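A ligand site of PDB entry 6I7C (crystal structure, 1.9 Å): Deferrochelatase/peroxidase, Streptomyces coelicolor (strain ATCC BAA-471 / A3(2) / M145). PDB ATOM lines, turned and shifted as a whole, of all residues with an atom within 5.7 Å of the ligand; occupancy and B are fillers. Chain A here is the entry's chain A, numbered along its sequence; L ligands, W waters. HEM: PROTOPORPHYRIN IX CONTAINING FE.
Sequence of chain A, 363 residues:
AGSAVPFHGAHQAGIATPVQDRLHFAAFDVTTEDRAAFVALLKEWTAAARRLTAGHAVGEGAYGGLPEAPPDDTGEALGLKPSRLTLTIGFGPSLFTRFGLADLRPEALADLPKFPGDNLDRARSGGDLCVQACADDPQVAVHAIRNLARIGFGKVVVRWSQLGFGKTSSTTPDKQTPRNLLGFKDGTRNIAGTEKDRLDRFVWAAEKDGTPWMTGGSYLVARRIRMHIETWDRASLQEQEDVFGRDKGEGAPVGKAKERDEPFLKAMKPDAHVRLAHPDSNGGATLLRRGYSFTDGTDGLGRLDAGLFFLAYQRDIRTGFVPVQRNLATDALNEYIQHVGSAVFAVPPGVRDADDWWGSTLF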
ATOM      1  N   ASN A 180      32.900 -12.239   8.610  1.00  0.00           N
ATOM      2  CA  ASN A 180      33.107 -12.190  10.057  1.00  0.00           C
ATOM      3  C   ASN A 180      32.772 -13.550  10.679  1.00  0.00           C
ATOM      4  O   ASN A 180      32.367 -14.501   9.998  1.00  0.00           O
ATOM      5  CB  ASN A 180      32.278 -11.084  10.666  1.00  0.00           C
ATOM      6  CG  ASN A 180      30.803 -11.194  10.325  1.00  0.00           C
ATOM      7  OD1 ASN A 180      30.197 -12.277  10.413  1.00  0.00           O
ATOM      8  ND2 ASN A 180      30.232 -10.085   9.910  1.00  0.00           N
ATOM      9  N   LEU A 182      30.316 -14.420  12.404  1.00  0.00           N
ATOM     10  CA  LEU A 182      28.922 -14.817  12.257  1.00  0.00           C
ATOM     11  C   LEU A 182      28.659 -15.518  10.930  1.00  0.00           C
ATOM     12  O   LEU A 182      27.527 -15.987  10.701  1.00  0.00           O
ATOM     13  CB  LEU A 182      28.010 -13.595  12.393  1.00  0.00           C
ATOM     14  CG  LEU A 182      28.049 -12.900  13.782  1.00  0.00           C
ATOM     15  CD1 LEU A 182      26.947 -11.875  13.878  1.00  0.00           C
ATOM     16  CD2 LEU A 182      28.000 -13.869  14.925  1.00  0.00           C
ATOM     17  N   PHE A 184      28.854 -14.113   7.842  1.00  0.00           N
ATOM     18  CA  PHE A 184      28.366 -13.221   6.812  1.00  0.00           C
ATOM     19  C   PHE A 184      29.514 -12.415   6.216  1.00  0.00           C
ATOM     20  O   PHE A 184      30.417 -11.986   6.941  1.00  0.00           O
ATOM     21  CB  PHE A 184      27.318 -12.252   7.340  1.00  0.00           C
ATOM     22  CG  PHE A 184      25.936 -12.852   7.413  1.00  0.00           C
ATOM     23  CD1 PHE A 184      25.614 -13.778   8.389  1.00  0.00           C
ATOM     24  CD2 PHE A 184      24.969 -12.495   6.488  1.00  0.00           C
ATOM     25  CE1 PHE A 184      24.359 -14.369   8.444  1.00  0.00           C
ATOM     26  CE2 PHE A 184      23.692 -13.083   6.540  1.00  0.00           C
ATOM     27  CZ  PHE A 184      23.400 -14.017   7.520  1.00  0.00           C
ATOM     28  N   LYS A 185      29.460 -12.192   4.900  1.00  0.00           N
ATOM     29  CA  LYS A 185      30.379 -11.245   4.286  1.00  0.00           C
ATOM     30  C   LYS A 185      30.233  -9.888   4.955  1.00  0.00           C
ATOM     31  O   LYS A 185      29.131  -9.441   5.287  1.00  0.00           O
ATOM     32  CB  LYS A 185      30.089 -11.130   2.798  1.00  0.00           C
ATOM     33  CG  LYS A 185      30.429 -12.355   2.001  1.00  0.00           C
ATOM     34  CD  LYS A 185      29.933 -12.204   0.540  1.00  0.00           C
ATOM     35  CE  LYS A 185      30.330 -13.383  -0.304  1.00  0.00           C
ATOM     36  NZ  LYS A 185      29.827 -13.236  -1.725  1.00  0.00           N
ATOM     37  N   ASP A 186      31.364  -9.236   5.158  1.00  0.00           N
ATOM     38  CA  ASP A 186      31.428  -7.984   5.896  1.00  0.00           C
ATOM     39  C   ASP A 186      32.369  -7.069   5.130  1.00  0.00           C
ATOM     40  O   ASP A 186      33.567  -7.350   5.053  1.00  0.00           O
ATOM     41  CB  ASP A 186      31.944  -8.202   7.334  1.00  0.00           C
ATOM     42  CG  ASP A 186      31.460  -7.136   8.306  1.00  0.00           C
ATOM     43  OD1 ASP A 186      31.101  -6.018   7.858  1.00  0.00           O
ATOM     44  OD2 ASP A 186      31.407  -7.417   9.516  1.00  0.00           O
ATOM     45  N   GLY A 187      31.833  -5.995   4.545  1.00  0.00           N
ATOM     46  CA  GLY A 187      32.626  -5.051   3.786  1.00  0.00           C
ATOM     47  C   GLY A 187      32.093  -4.737   2.394  1.00  0.00           C
ATOM     48  O   GLY A 187      32.693  -3.942   1.659  1.00  0.00           O
ATOM     49  N   THR A 188      30.963  -5.324   2.033  1.00  0.00           N
ATOM     50  CA  THR A 188      30.463  -5.199   0.661  1.00  0.00           C
ATOM     51  C   THR A 188      30.235  -3.746   0.275  1.00  0.00           C
ATOM     52  O   THR A 188      30.766  -3.248  -0.731  1.00  0.00           O
ATOM     53  CB  THR A 188      29.162  -5.975   0.530  1.00  0.00           C
ATOM     54  OG1 THR A 188      29.350  -7.355   0.845  1.00  0.00           O
ATOM     55  CG2 THR A 188      28.592  -5.828  -0.923  1.00  0.00           C
ATOM     56  N   ARG A 189      29.430  -3.019   1.060  1.00  0.00           N
ATOM     57  CA  ARG A 189      29.144  -1.599   0.782  1.00  0.00           C
ATOM     58  C   ARG A 189      29.925  -0.744   1.776  1.00  0.00           C
ATOM     59  O   ARG A 189      29.429  -0.346   2.812  1.00  0.00           O
ATOM     60  CB  ARG A 189      27.641  -1.333   0.855  1.00  0.00           C
ATOM     61  CG  ARG A 189      26.900  -1.670  -0.434  1.00  0.00           C
ATOM     62  CD  ARG A 189      25.384  -1.313  -0.366  1.00  0.00           C
ATOM     63  NE  ARG A 189      25.205  -0.084   0.398  1.00  0.00           N
ATOM     64  CZ  ARG A 189      25.360   1.146  -0.093  1.00  0.00           C
ATOM     65  NH1 ARG A 189      25.212   2.184   0.702  1.00  0.00           N
ATOM     66  NH2 ARG A 189      25.636   1.332  -1.384  1.00  0.00           N
ATOM     67  N   ASN A 190      31.176  -0.530   1.474  1.00  0.00           N
ATOM     68  CA  ASN A 190      32.104   0.283   2.216  1.00  0.00           C
ATOM     69  C   ASN A 190      32.594   1.388   1.264  1.00  0.00           C
ATOM     70  O   ASN A 190      32.112   1.514   0.140  1.00  0.00           O
ATOM     71  CB  ASN A 190      33.250  -0.583   2.763  1.00  0.00           C
ATOM     72  CG  ASN A 190      33.982   0.072   3.904  1.00  0.00           C
ATOM     73  OD1 ASN A 190      33.399   0.830   4.691  1.00  0.00           O
ATOM     74  ND2 ASN A 190      35.265  -0.241   4.033  1.00  0.00           N
ATOM     75  N   ILE A 225      33.701  -5.437  20.194  1.00  0.00           N
ATOM     76  CA  ILE A 225      32.346  -5.985  20.215  1.00  0.00           C
ATOM     77  C   ILE A 225      32.389  -7.489  20.402  1.00  0.00           C
ATOM     78  O   ILE A 225      32.864  -8.211  19.518  1.00  0.00           O
ATOM     79  CB  ILE A 225      31.560  -5.614  18.956  1.00  0.00           C
ATOM     80  CG1 ILE A 225      31.531  -4.084  18.784  1.00  0.00           C
ATOM     81  CG2 ILE A 225      30.151  -6.162  19.028  1.00  0.00           C
ATOM     82  CD1 ILE A 225      30.905  -3.615  17.490  1.00  0.00           C
ATOM     83  N   MET A 227      30.691 -11.145  20.499  1.00  0.00           N
ATOM     84  CA  MET A 227      29.601 -11.826  19.821  1.00  0.00           C
ATOM     85  C   MET A 227      29.099 -12.988  20.675  1.00  0.00           C
ATOM     86  O   MET A 227      29.894 -13.799  21.175  1.00  0.00           O
ATOM     87  CB  MET A 227      30.041 -12.377  18.457  1.00  0.00           C
ATOM     88  CG  MET A 227      30.242 -11.316  17.410  1.00  0.00           C
ATOM     89  SD  MET A 227      31.289 -12.006  16.100  1.00  0.00           S
ATOM     90  CE  MET A 227      31.139 -10.698  14.920  1.00  0.00           C
ATOM     91  N   PHE A 244      20.320  -9.379   9.201  1.00  0.00           N
ATOM     92  CA  PHE A 244      21.148  -8.504   8.381  1.00  0.00           C
ATOM     93  C   PHE A 244      20.408  -7.913   7.189  1.00  0.00           C
ATOM     94  O   PHE A 244      20.662  -6.766   6.821  1.00  0.00           O
ATOM     95  CB  PHE A 244      22.383  -9.247   7.874  1.00  0.00           C
ATOM     96  CG  PHE A 244      23.357  -9.506   8.951  1.00  0.00           C
ATOM     97  CD1 PHE A 244      24.063  -8.455   9.520  1.00  0.00           C
ATOM     98  CD2 PHE A 244      23.587 -10.773   9.405  1.00  0.00           C
ATOM     99  CE1 PHE A 244      24.919  -8.684  10.559  1.00  0.00           C
ATOM    100  CE2 PHE A 244      24.476 -11.007  10.428  1.00  0.00           C
ATOM    101  CZ  PHE A 244      25.137  -9.953  11.000  1.00  0.00           C
ATOM    102  N   ARG A 246      20.554  -9.585   4.253  1.00  0.00           N
ATOM    103  CA  ARG A 246      21.290 -10.183   3.140  1.00  0.00           C
ATOM    104  C   ARG A 246      21.283 -11.680   3.380  1.00  0.00           C
ATOM    105  O   ARG A 246      21.152 -12.138   4.521  1.00  0.00           O
ATOM    106  CB  ARG A 246      22.705  -9.690   3.023  1.00  0.00           C
ATOM    107  CG  ARG A 246      22.869  -8.230   2.665  1.00  0.00           C
ATOM    108  CD  ARG A 246      24.330  -7.844   2.599  1.00  0.00           C
ATOM    109  NE  ARG A 246      24.553  -6.481   2.131  1.00  0.00           N
ATOM    110  CZ  ARG A 246      24.759  -6.160   0.849  1.00  0.00           C
ATOM    111  NH1 ARG A 246      24.764  -7.096  -0.095  1.00  0.00           N
ATOM    112  NH2 ARG A 246      24.988  -4.896   0.506  1.00  0.00           N
ATOM    113  N   PRO A 263      21.043  -2.803  -2.469  1.00  0.00           N
ATOM    114  CA  PRO A 263      19.935  -3.182  -1.565  1.00  0.00           C
ATOM    115  C   PRO A 263      18.641  -2.461  -1.936  1.00  0.00           C
ATOM    116  O   PRO A 263      18.655  -1.305  -2.336  1.00  0.00           O
ATOM    117  CB  PRO A 263      20.433  -2.739  -0.187  1.00  0.00           C
ATOM    118  CG  PRO A 263      21.885  -2.513  -0.319  1.00  0.00           C
ATOM    119  CD  PRO A 263      22.142  -2.122  -1.759  1.00  0.00           C
ATOM    120  N   HIS A 273      19.881  -5.004  10.173  1.00  0.00           N
ATOM    121  CA  HIS A 273      21.107  -4.247  10.330  1.00  0.00           C
ATOM    122  C   HIS A 273      21.392  -3.370   9.109  1.00  0.00           C
ATOM    123  O   HIS A 273      21.653  -2.185   9.265  1.00  0.00           O
ATOM    124  CB  HIS A 273      22.255  -5.203  10.595  1.00  0.00           C
ATOM    125  CG  HIS A 273      23.558  -4.527  10.871  1.00  0.00           C
ATOM    126  ND1 HIS A 273      23.773  -3.823  12.028  1.00  0.00           N
ATOM    127  CD2 HIS A 273      24.707  -4.444  10.154  1.00  0.00           C
ATOM    128  CE1 HIS A 273      25.005  -3.350  12.040  1.00  0.00           C
ATOM    129  NE2 HIS A 273      25.588  -3.686  10.902  1.00  0.00           N
ATOM    130  N   VAL A 274      21.381  -3.949   7.897  1.00  0.00           N
ATOM    131  CA  VAL A 274      21.748  -3.178   6.723  1.00  0.00           C
ATOM    132  C   VAL A 274      20.754  -2.042   6.510  1.00  0.00           C
ATOM    133  O   VAL A 274      21.123  -0.912   6.181  1.00  0.00           O
ATOM    134  CB  VAL A 274      21.840  -4.088   5.491  1.00  0.00           C
ATOM    135  CG1 VAL A 274      21.928  -3.278   4.189  1.00  0.00           C
ATOM    136  CG2 VAL A 274      23.028  -5.013   5.592  1.00  0.00           C
ATOM    137  N   ALA A 277      21.639   0.705   9.047  1.00  0.00           N
ATOM    138  CA  ALA A 277      22.969   1.293   8.953  1.00  0.00           C
ATOM    139  C   ALA A 277      23.223   1.964   7.608  1.00  0.00           C
ATOM    140  O   ALA A 277      24.244   2.654   7.458  1.00  0.00           O
ATOM    141  CB  ALA A 277      24.027   0.213   9.223  1.00  0.00           C
ATOM    142  N   HIS A 278      22.335   1.759   6.649  1.00  0.00           N
ATOM    143  CA  HIS A 278      22.503   2.291   5.307  1.00  0.00           C
ATOM    144  C   HIS A 278      22.527   3.811   5.327  1.00  0.00           C
ATOM    145  O   HIS A 278      21.825   4.438   6.122  1.00  0.00           O
ATOM    146  CB  HIS A 278      21.360   1.789   4.422  1.00  0.00           C
ATOM    147  CG  HIS A 278      21.591   2.000   2.952  1.00  0.00           C
ATOM    148  ND1 HIS A 278      21.348   3.212   2.328  1.00  0.00           N
ATOM    149  CD2 HIS A 278      22.036   1.157   1.992  1.00  0.00           C
ATOM    150  CE1 HIS A 278      21.629   3.085   1.043  1.00  0.00           C
ATOM    151  NE2 HIS A 278      22.051   1.857   0.810  1.00  0.00           N
ATOM    152  N   PRO A 279      23.349   4.446   4.486  1.00  0.00           N
ATOM    153  CA  PRO A 279      23.383   5.918   4.473  1.00  0.00           C
ATOM    154  C   PRO A 279      22.016   6.571   4.256  1.00  0.00           C
ATOM    155  O   PRO A 279      21.717   7.601   4.891  1.00  0.00           O
ATOM    156  CB  PRO A 279      24.324   6.223   3.309  1.00  0.00           C
ATOM    157  CG  PRO A 279      25.212   5.045   3.204  1.00  0.00           C
ATOM    158  CD  PRO A 279      24.344   3.844   3.562  1.00  0.00           C
ATOM    159  N   LEU A 287      30.482   5.663   6.324  1.00  0.00           N
ATOM    160  CA  LEU A 287      31.686   5.370   7.093  1.00  0.00           C
ATOM    161  C   LEU A 287      32.667   4.556   6.270  1.00  0.00           C
ATOM    162  O   LEU A 287      32.282   3.853   5.339  1.00  0.00           O
ATOM    163  CB  LEU A 287      31.351   4.552   8.351  1.00  0.00           C
ATOM    164  CG  LEU A 287      30.308   5.067   9.321  1.00  0.00           C
ATOM    165  CD1 LEU A 287      29.997   3.975  10.326  1.00  0.00           C
ATOM    166  CD2 LEU A 287      30.822   6.329  10.017  1.00  0.00           C
ATOM    167  N   ARG A 289      34.655   1.488   7.076  1.00  0.00           N
ATOM    168  CA  ARG A 289      34.854   0.426   8.051  1.00  0.00           C
ATOM    169  C   ARG A 289      36.136  -0.351   7.754  1.00  0.00           C
ATOM    170  O   ARG A 289      36.405  -0.682   6.591  1.00  0.00           O
ATOM    171  CB  ARG A 289      33.640  -0.515   8.013  1.00  0.00           C
ATOM    172  CG  ARG A 289      32.373   0.176   8.520  1.00  0.00           C
ATOM    173  CD  ARG A 289      31.134  -0.721   8.329  1.00  0.00           C
ATOM    174  NE  ARG A 289      30.771  -0.817   6.942  1.00  0.00           N
ATOM    175  CZ  ARG A 289      30.414  -1.942   6.336  1.00  0.00           C
ATOM    176  NH1 ARG A 289      30.368  -3.095   7.006  1.00  0.00           N
ATOM    177  NH2 ARG A 289      30.121  -1.908   5.034  1.00  0.00           N
ATOM    178  N   LEU A 308      34.398  -8.925  17.222  1.00  0.00           N
ATOM    179  CA  LEU A 308      34.776  -8.088  16.106  1.00  0.00           C
ATOM    180  C   LEU A 308      35.343  -6.817  16.710  1.00  0.00           C
ATOM    181  O   LEU A 308      34.717  -6.189  17.569  1.00  0.00           O
ATOM    182  CB  LEU A 308      33.600  -7.812  15.209  1.00  0.00           C
ATOM    183  CG  LEU A 308      33.905  -7.237  13.833  1.00  0.00           C
ATOM    184  CD1 LEU A 308      32.877  -7.750  12.824  1.00  0.00           C
ATOM    185  CD2 LEU A 308      33.863  -5.736  13.911  1.00  0.00           C
ATOM    186  N   PHE A 310      35.795  -3.419  15.883  1.00  0.00           N
ATOM    187  CA  PHE A 310      35.212  -2.542  14.865  1.00  0.00           C
ATOM    188  C   PHE A 310      36.027  -1.272  14.810  1.00  0.00           C
ATOM    189  O   PHE A 310      36.337  -0.687  15.851  1.00  0.00           O
ATOM    190  CB  PHE A 310      33.755  -2.235  15.256  1.00  0.00           C
ATOM    191  CG  PHE A 310      33.040  -1.349  14.297  1.00  0.00           C
ATOM    192  CD1 PHE A 310      32.391  -1.883  13.190  1.00  0.00           C
ATOM    193  CD2 PHE A 310      32.991   0.014  14.505  1.00  0.00           C
ATOM    194  CE1 PHE A 310      31.717  -1.050  12.316  1.00  0.00           C
ATOM    195  CE2 PHE A 310      32.323   0.835  13.610  1.00  0.00           C
ATOM    196  CZ  PHE A 310      31.696   0.305  12.538  1.00  0.00           C
ATOM    197  N   PHE A 321      29.931   8.042  12.856  1.00  0.00           N
ATOM    198  CA  PHE A 321      29.589   6.932  13.742  1.00  0.00           C
ATOM    199  C   PHE A 321      28.373   7.227  14.612  1.00  0.00           C
ATOM    200  O   PHE A 321      27.519   6.357  14.806  1.00  0.00           O
ATOM    201  CB  PHE A 321      30.779   6.580  14.615  1.00  0.00           C
ATOM    202  CG  PHE A 321      30.516   5.436  15.553  1.00  0.00           C
ATOM    203  CD1 PHE A 321      30.653   4.133  15.131  1.00  0.00           C
ATOM    204  CD2 PHE A 321      30.130   5.683  16.850  1.00  0.00           C
ATOM    205  CE1 PHE A 321      30.399   3.088  16.017  1.00  0.00           C
ATOM    206  CE2 PHE A 321      29.879   4.661  17.729  1.00  0.00           C
ATOM    207  CZ  PHE A 321      30.006   3.361  17.316  1.00  0.00           C
ATOM    208  N   VAL A 324      24.789   6.906  12.985  1.00  0.00           N
ATOM    209  CA  VAL A 324      24.566   5.522  12.575  1.00  0.00           C
ATOM    210  C   VAL A 324      24.356   4.634  13.798  1.00  0.00           C
ATOM    211  O   VAL A 324      23.371   3.896  13.899  1.00  0.00           O
ATOM    212  CB  VAL A 324      25.726   5.024  11.699  1.00  0.00           C
ATOM    213  CG1 VAL A 324      25.550   3.560  11.371  1.00  0.00           C
ATOM    214  CG2 VAL A 324      25.811   5.869  10.409  1.00  0.00           C
ATOM    215  N   GLN A 325      25.284   4.696  14.762  1.00  0.00           N
ATOM    216  CA  GLN A 325      25.130   3.873  15.970  1.00  0.00           C
ATOM    217  C   GLN A 325      23.857   4.225  16.723  1.00  0.00           C
ATOM    218  O   GLN A 325      23.197   3.342  17.296  1.00  0.00           O
ATOM    219  CB  GLN A 325      26.366   4.034  16.863  1.00  0.00           C
ATOM    220  CG  GLN A 325      26.316   3.247  18.174  1.00  0.00           C
ATOM    221  CD  GLN A 325      26.267   1.728  17.977  1.00  0.00           C
ATOM    222  OE1 GLN A 325      26.772   1.207  17.003  1.00  0.00           O
ATOM    223  NE2 GLN A 325      25.642   1.029  18.909  1.00  0.00           N
ATOM    224  N   LEU A 328      21.122   2.260  15.260  1.00  0.00           N
ATOM    225  CA  LEU A 328      21.183   0.828  15.569  1.00  0.00           C
ATOM    226  C   LEU A 328      20.581   0.480  16.941  1.00  0.00           C
ATOM    227  O   LEU A 328      20.685  -0.686  17.392  1.00  0.00           O
ATOM    228  CB  LEU A 328      22.631   0.344  15.508  1.00  0.00           C
ATOM    229  CG  LEU A 328      23.313   0.580  14.161  1.00  0.00           C
ATOM    230  CD1 LEU A 328      24.733  -0.015  14.157  1.00  0.00           C
ATOM    231  CD2 LEU A 328      22.484  -0.020  13.037  1.00  0.00           C
ATOM    232  N   LEU A 333      20.497  -7.134  15.309  1.00  0.00           N
ATOM    233  CA  LEU A 333      21.809  -7.676  15.679  1.00  0.00           C
ATOM    234  C   LEU A 333      22.093  -7.515  17.169  1.00  0.00           C
ATOM    235  O   LEU A 333      22.891  -8.270  17.735  1.00  0.00           O
ATOM    236  CB  LEU A 333      22.893  -6.957  14.870  1.00  0.00           C
ATOM    237  CG  LEU A 333      24.328  -7.466  14.989  1.00  0.00           C
ATOM    238  CD1 LEU A 333      24.461  -8.909  14.565  1.00  0.00           C
ATOM    239  CD2 LEU A 333      25.243  -6.563  14.177  1.00  0.00           C
ATOM    240  N   ILE A 337      25.204  -9.351  20.130  1.00  0.00           N
ATOM    241  CA  ILE A 337      26.487  -8.669  20.312  1.00  0.00           C
ATOM    242  C   ILE A 337      26.442  -7.829  21.577  1.00  0.00           C
ATOM    243  O   ILE A 337      25.371  -7.536  22.126  1.00  0.00           O
ATOM    244  CB  ILE A 337      26.862  -7.779  19.108  1.00  0.00           C
ATOM    245  CG1 ILE A 337      25.853  -6.640  18.934  1.00  0.00           C
ATOM    246  CG2 ILE A 337      26.921  -8.579  17.839  1.00  0.00           C
ATOM    247  CD1 ILE A 337      26.366  -5.497  18.081  1.00  0.00           C
ATOM    248  N   HIS A 339      28.881  -4.309  22.954  1.00  0.00           N
ATOM    249  CA  HIS A 339      30.044  -3.422  22.938  1.00  0.00           C
ATOM    250  C   HIS A 339      30.688  -3.410  24.316  1.00  0.00           C
ATOM    251  O   HIS A 339      30.028  -3.072  25.318  1.00  0.00           O
ATOM    252  CB  HIS A 339      29.659  -2.019  22.509  1.00  0.00           C
ATOM    253  CG  HIS A 339      29.100  -1.937  21.113  1.00  0.00           C
ATOM    254  ND1 HIS A 339      29.625  -1.100  20.145  1.00  0.00           N
ATOM    255  CD2 HIS A 339      28.051  -2.568  20.539  1.00  0.00           C
ATOM    256  CE1 HIS A 339      28.926  -1.224  19.033  1.00  0.00           C
ATOM    257  NE2 HIS A 339      27.958  -2.101  19.248  1.00  0.00           N
HETATM  258  CHA HEM L   1      26.977  -3.622   6.904  1.00  0.00           C
HETATM  259  CHB HEM L   1      27.887  -7.102  10.124  1.00  0.00           C
HETATM  260  CHC HEM L   1      28.592  -3.705  13.478  1.00  0.00           C
HETATM  261  CHD HEM L   1      27.789  -0.233  10.215  1.00  0.00           C
HETATM  262  C1A HEM L   1      27.094  -4.855   7.483  1.00  0.00           C
HETATM  263  C2A HEM L   1      26.949  -6.129   6.801  1.00  0.00           C
HETATM  264  C3A HEM L   1      27.206  -7.094   7.702  1.00  0.00           C
HETATM  265  C4A HEM L   1      27.525  -6.450   8.964  1.00  0.00           C
HETATM  266  CMA HEM L   1      27.135  -8.611   7.501  1.00  0.00           C
HETATM  267  CAA HEM L   1      26.528  -6.353   5.332  1.00  0.00           C
HETATM  268  CBA HEM L   1      27.725  -6.346   4.423  1.00  0.00           C
HETATM  269  CGA HEM L   1      28.422  -5.019   4.260  1.00  0.00           C
HETATM  270  O1A HEM L   1      27.967  -4.164   3.446  1.00  0.00           O
HETATM  271  O2A HEM L   1      29.450  -4.804   4.907  1.00  0.00           O
HETATM  272  C1B HEM L   1      28.168  -6.471  11.327  1.00  0.00           C
HETATM  273  C2B HEM L   1      28.552  -7.150  12.561  1.00  0.00           C
HETATM  274  C3B HEM L   1      28.748  -6.216  13.499  1.00  0.00           C
HETATM  275  C4B HEM L   1      28.508  -4.923  12.872  1.00  0.00           C
HETATM  276  CMB HEM L   1      28.655  -8.666  12.676  1.00  0.00           C
HETATM  277  CAB HEM L   1      29.168  -6.409  14.983  1.00  0.00           C
HETATM  278  CBB HEM L   1      29.616  -7.571  15.443  1.00  0.00           C
HETATM  279  C1C HEM L   1      28.423  -2.477  12.910  1.00  0.00           C
HETATM  280  C2C HEM L   1      28.515  -1.194  13.584  1.00  0.00           C
HETATM  281  C3C HEM L   1      28.279  -0.237  12.665  1.00  0.00           C
HETATM  282  C4C HEM L   1      28.041  -0.884  11.407  1.00  0.00           C
HETATM  283  CMC HEM L   1      28.799  -1.012  15.086  1.00  0.00           C
HETATM  284  CAC HEM L   1      28.220   1.292  12.834  1.00  0.00           C
HETATM  285  CBC HEM L   1      27.942   1.839  14.012  1.00  0.00           C
HETATM  286  C1D HEM L   1      27.566  -0.843   9.024  1.00  0.00           C
HETATM  287  C2D HEM L   1      27.349  -0.173   7.748  1.00  0.00           C
HETATM  288  C3D HEM L   1      27.097  -1.114   6.840  1.00  0.00           C
HETATM  289  C4D HEM L   1      27.160  -2.415   7.506  1.00  0.00           C
HETATM  290  CMD HEM L   1      27.391   1.341   7.495  1.00  0.00           C
HETATM  291  CAD HEM L   1      26.823  -0.879   5.355  1.00  0.00           C
HETATM  292  CBD HEM L   1      25.332  -0.655   5.111  1.00  0.00           C
HETATM  293  CGD HEM L   1      25.166  -0.263   3.637  1.00  0.00           C
HETATM  294  O1D HEM L   1      25.507   0.890   3.274  1.00  0.00           O
HETATM  295  O2D HEM L   1      24.688  -1.083   2.872  1.00  0.00           O
HETATM  296  NA  HEM L   1      27.451  -5.085   8.801  1.00  0.00           N
HETATM  297  NB  HEM L   1      28.188  -5.144  11.564  1.00  0.00           N
HETATM  298  NC  HEM L   1      28.142  -2.243  11.576  1.00  0.00           N
HETATM  299  ND  HEM L   1      27.427  -2.201   8.835  1.00  0.00           N
HETATM  300 FE   HEM L   1      27.700  -3.686  10.236  1.00  0.00          FE
HETATM  301  O   HOH W   1      25.278  -3.844   3.010  1.00  0.00           O
HETATM  302  O   HOH W   2      27.854   1.984   3.270  1.00  0.00           O
HETATM  303  O   HOH W   3      28.611   3.591   5.484  1.00  0.00           O
HETATM  304  O   HOH W   4      31.584  -5.551  11.212  1.00  0.00           O
HETATM  305  O   HOH W   5      26.397   4.390   6.995  1.00  0.00           O
HETATM  306  O   HOH W   6      26.194  -1.873  17.112  1.00  0.00           O
HETATM  307  O   HOH W   7      30.049  -3.924   9.702  1.00  0.00           O
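The backbone carbonyl oxygen (O) of Arg 189 sits at hydrogen-bond distance from the guanidinium group (NH2) of Arg 289 (2.8 Å).
NE2 of His 278 sits at hydrogen-bond distance from NH1 of Arg 189, at 3.2 Å.
OD1 of Asp 186 lies within salt-bridge range of NH1 of Arg 289.
The backbone NH of Arg 289 sits at hydrogen-bond distance from the side-chain amide oxygen of Asn 190, 2.8 Å away.
O of Phe 244 lies within hydrogen-bond range of N of Val 274 (3.1 Å).
The side-chain amide nitrogen (ND2) of Asn 180 sits at hydrogen-bond distance from the side-chain carboxylate (OD2) of Asp 186.
N of Phe 184 sits at hydrogen-bond distance from OD1 of Asn 180, at 3.4 Å.
N of Leu 308 lies within hydrogen-bond range of O of Ile 225, at 2.9 Å.
Water W7 bridges NH1 of Arg 289 (2.8 Å) and OD1 of Asp 186 (3.0 Å).
Water W2 lies within hydrogen-bond range of O1D of the ligand (2.6 Å) and O of Arg 189 (2.8 Å).
Water W1 lies within hydrogen-bond range of NH2 of Arg 246 (2.7 Å) and O1A of the ligand (2.7 Å).
Water W6 lies within hydrogen-bond range of a ring nitrogen (NE2) of His 339 and the side-chain amide oxygen (OE1) of Gln 325.
FE of the ligand is bound by NE2 of His 273 (2.2 Å).
The backbone NH of Gly 187 lies within hydrogen-bond range of an oxygen (O2A) of the ligand, at 2.7 Å.
The backbone NH of Arg 189 lies within hydrogen-bond range of an oxygen (O1A) of the ligand, at 3.0 Å.
An oxygen (O2D) of the ligand lies within salt-bridge range of the guanidinium group of Arg 189.
O2A of the ligand is in salt-bridge range of NH1 of Arg 289, 2.9 Å away.
The backbone NH (N) of Thr 188 sits at hydrogen-bond distance from an oxygen (O2A) of the ligand (3.3 Å).
Asn 180 touches the ligand.
Leu 182 touches the ligand (CD1 to CMB, 3.8 Å).
Phe 184 touches the ligand.
Lys 185 touches the ligand (O to CMA, 3.1 Å).
Asp 186 touches the ligand.
CG2 of Ile 225 touches CBB of the ligand, at 3.9 Å.
Met 227 touches the ligand.
Phe 244 touches the ligand.
Arg 246 touches the ligand (NE to CAA, 3.8 Å).
Val 274 touches the ligand (CG2 to CAA, 3.8 Å).
Ala 277 touches the ligand (O to CMD, 3.4 Å).
CD2 of His 278 touches O2D of the ligand (3.6 Å).
Pro 279 touches the ligand (CD to O1D, 3.2 Å).
CB of Leu 308 touches CBB of the ligand, at 3.998 Å.
Phe 310 touches the ligand (CE1 to C2C, 3.4 Å).
Phe 321 touches the ligand (CE1 to CBC, 3.4 Å).
Val 324 touches the ligand.
Gln 325 touches the ligand.
CD1 of Leu 328 touches CBC of the ligand (3.7 Å).
Leu 333 touches the ligand.
CG2 of Ile 337 touches CBB of the ligand, 3.7 Å away.
His 339 touches the ligand (CE1 to CMC, 3.95 Å).
Hydrophobic or aromatic side chains within 4 Å of the ligand: Leu 182, Phe 184, Ile 225, Met 227, Phe 244, His 273, Val 274, Ala 277, His 278, Pro 279, Leu 308, Phe 310, Phe 321, Val 324, Leu 328, Leu 333, Ile 337 and His 339.
Within 4 Å of the ligand: Asn 180, Leu 182, Phe 184, Lys 185, Asp 186, Gly 187, Thr 188, Arg 189, Ile 225, Met 227, Phe 244, Arg 246, His 273, Val 274, Ala 277, His 278, Pro 279, Arg 289, Leu 308, Phe 310, Phe 321, Val 324, Gln 325, Leu 328, Leu 333, Ile 337 and His 339.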
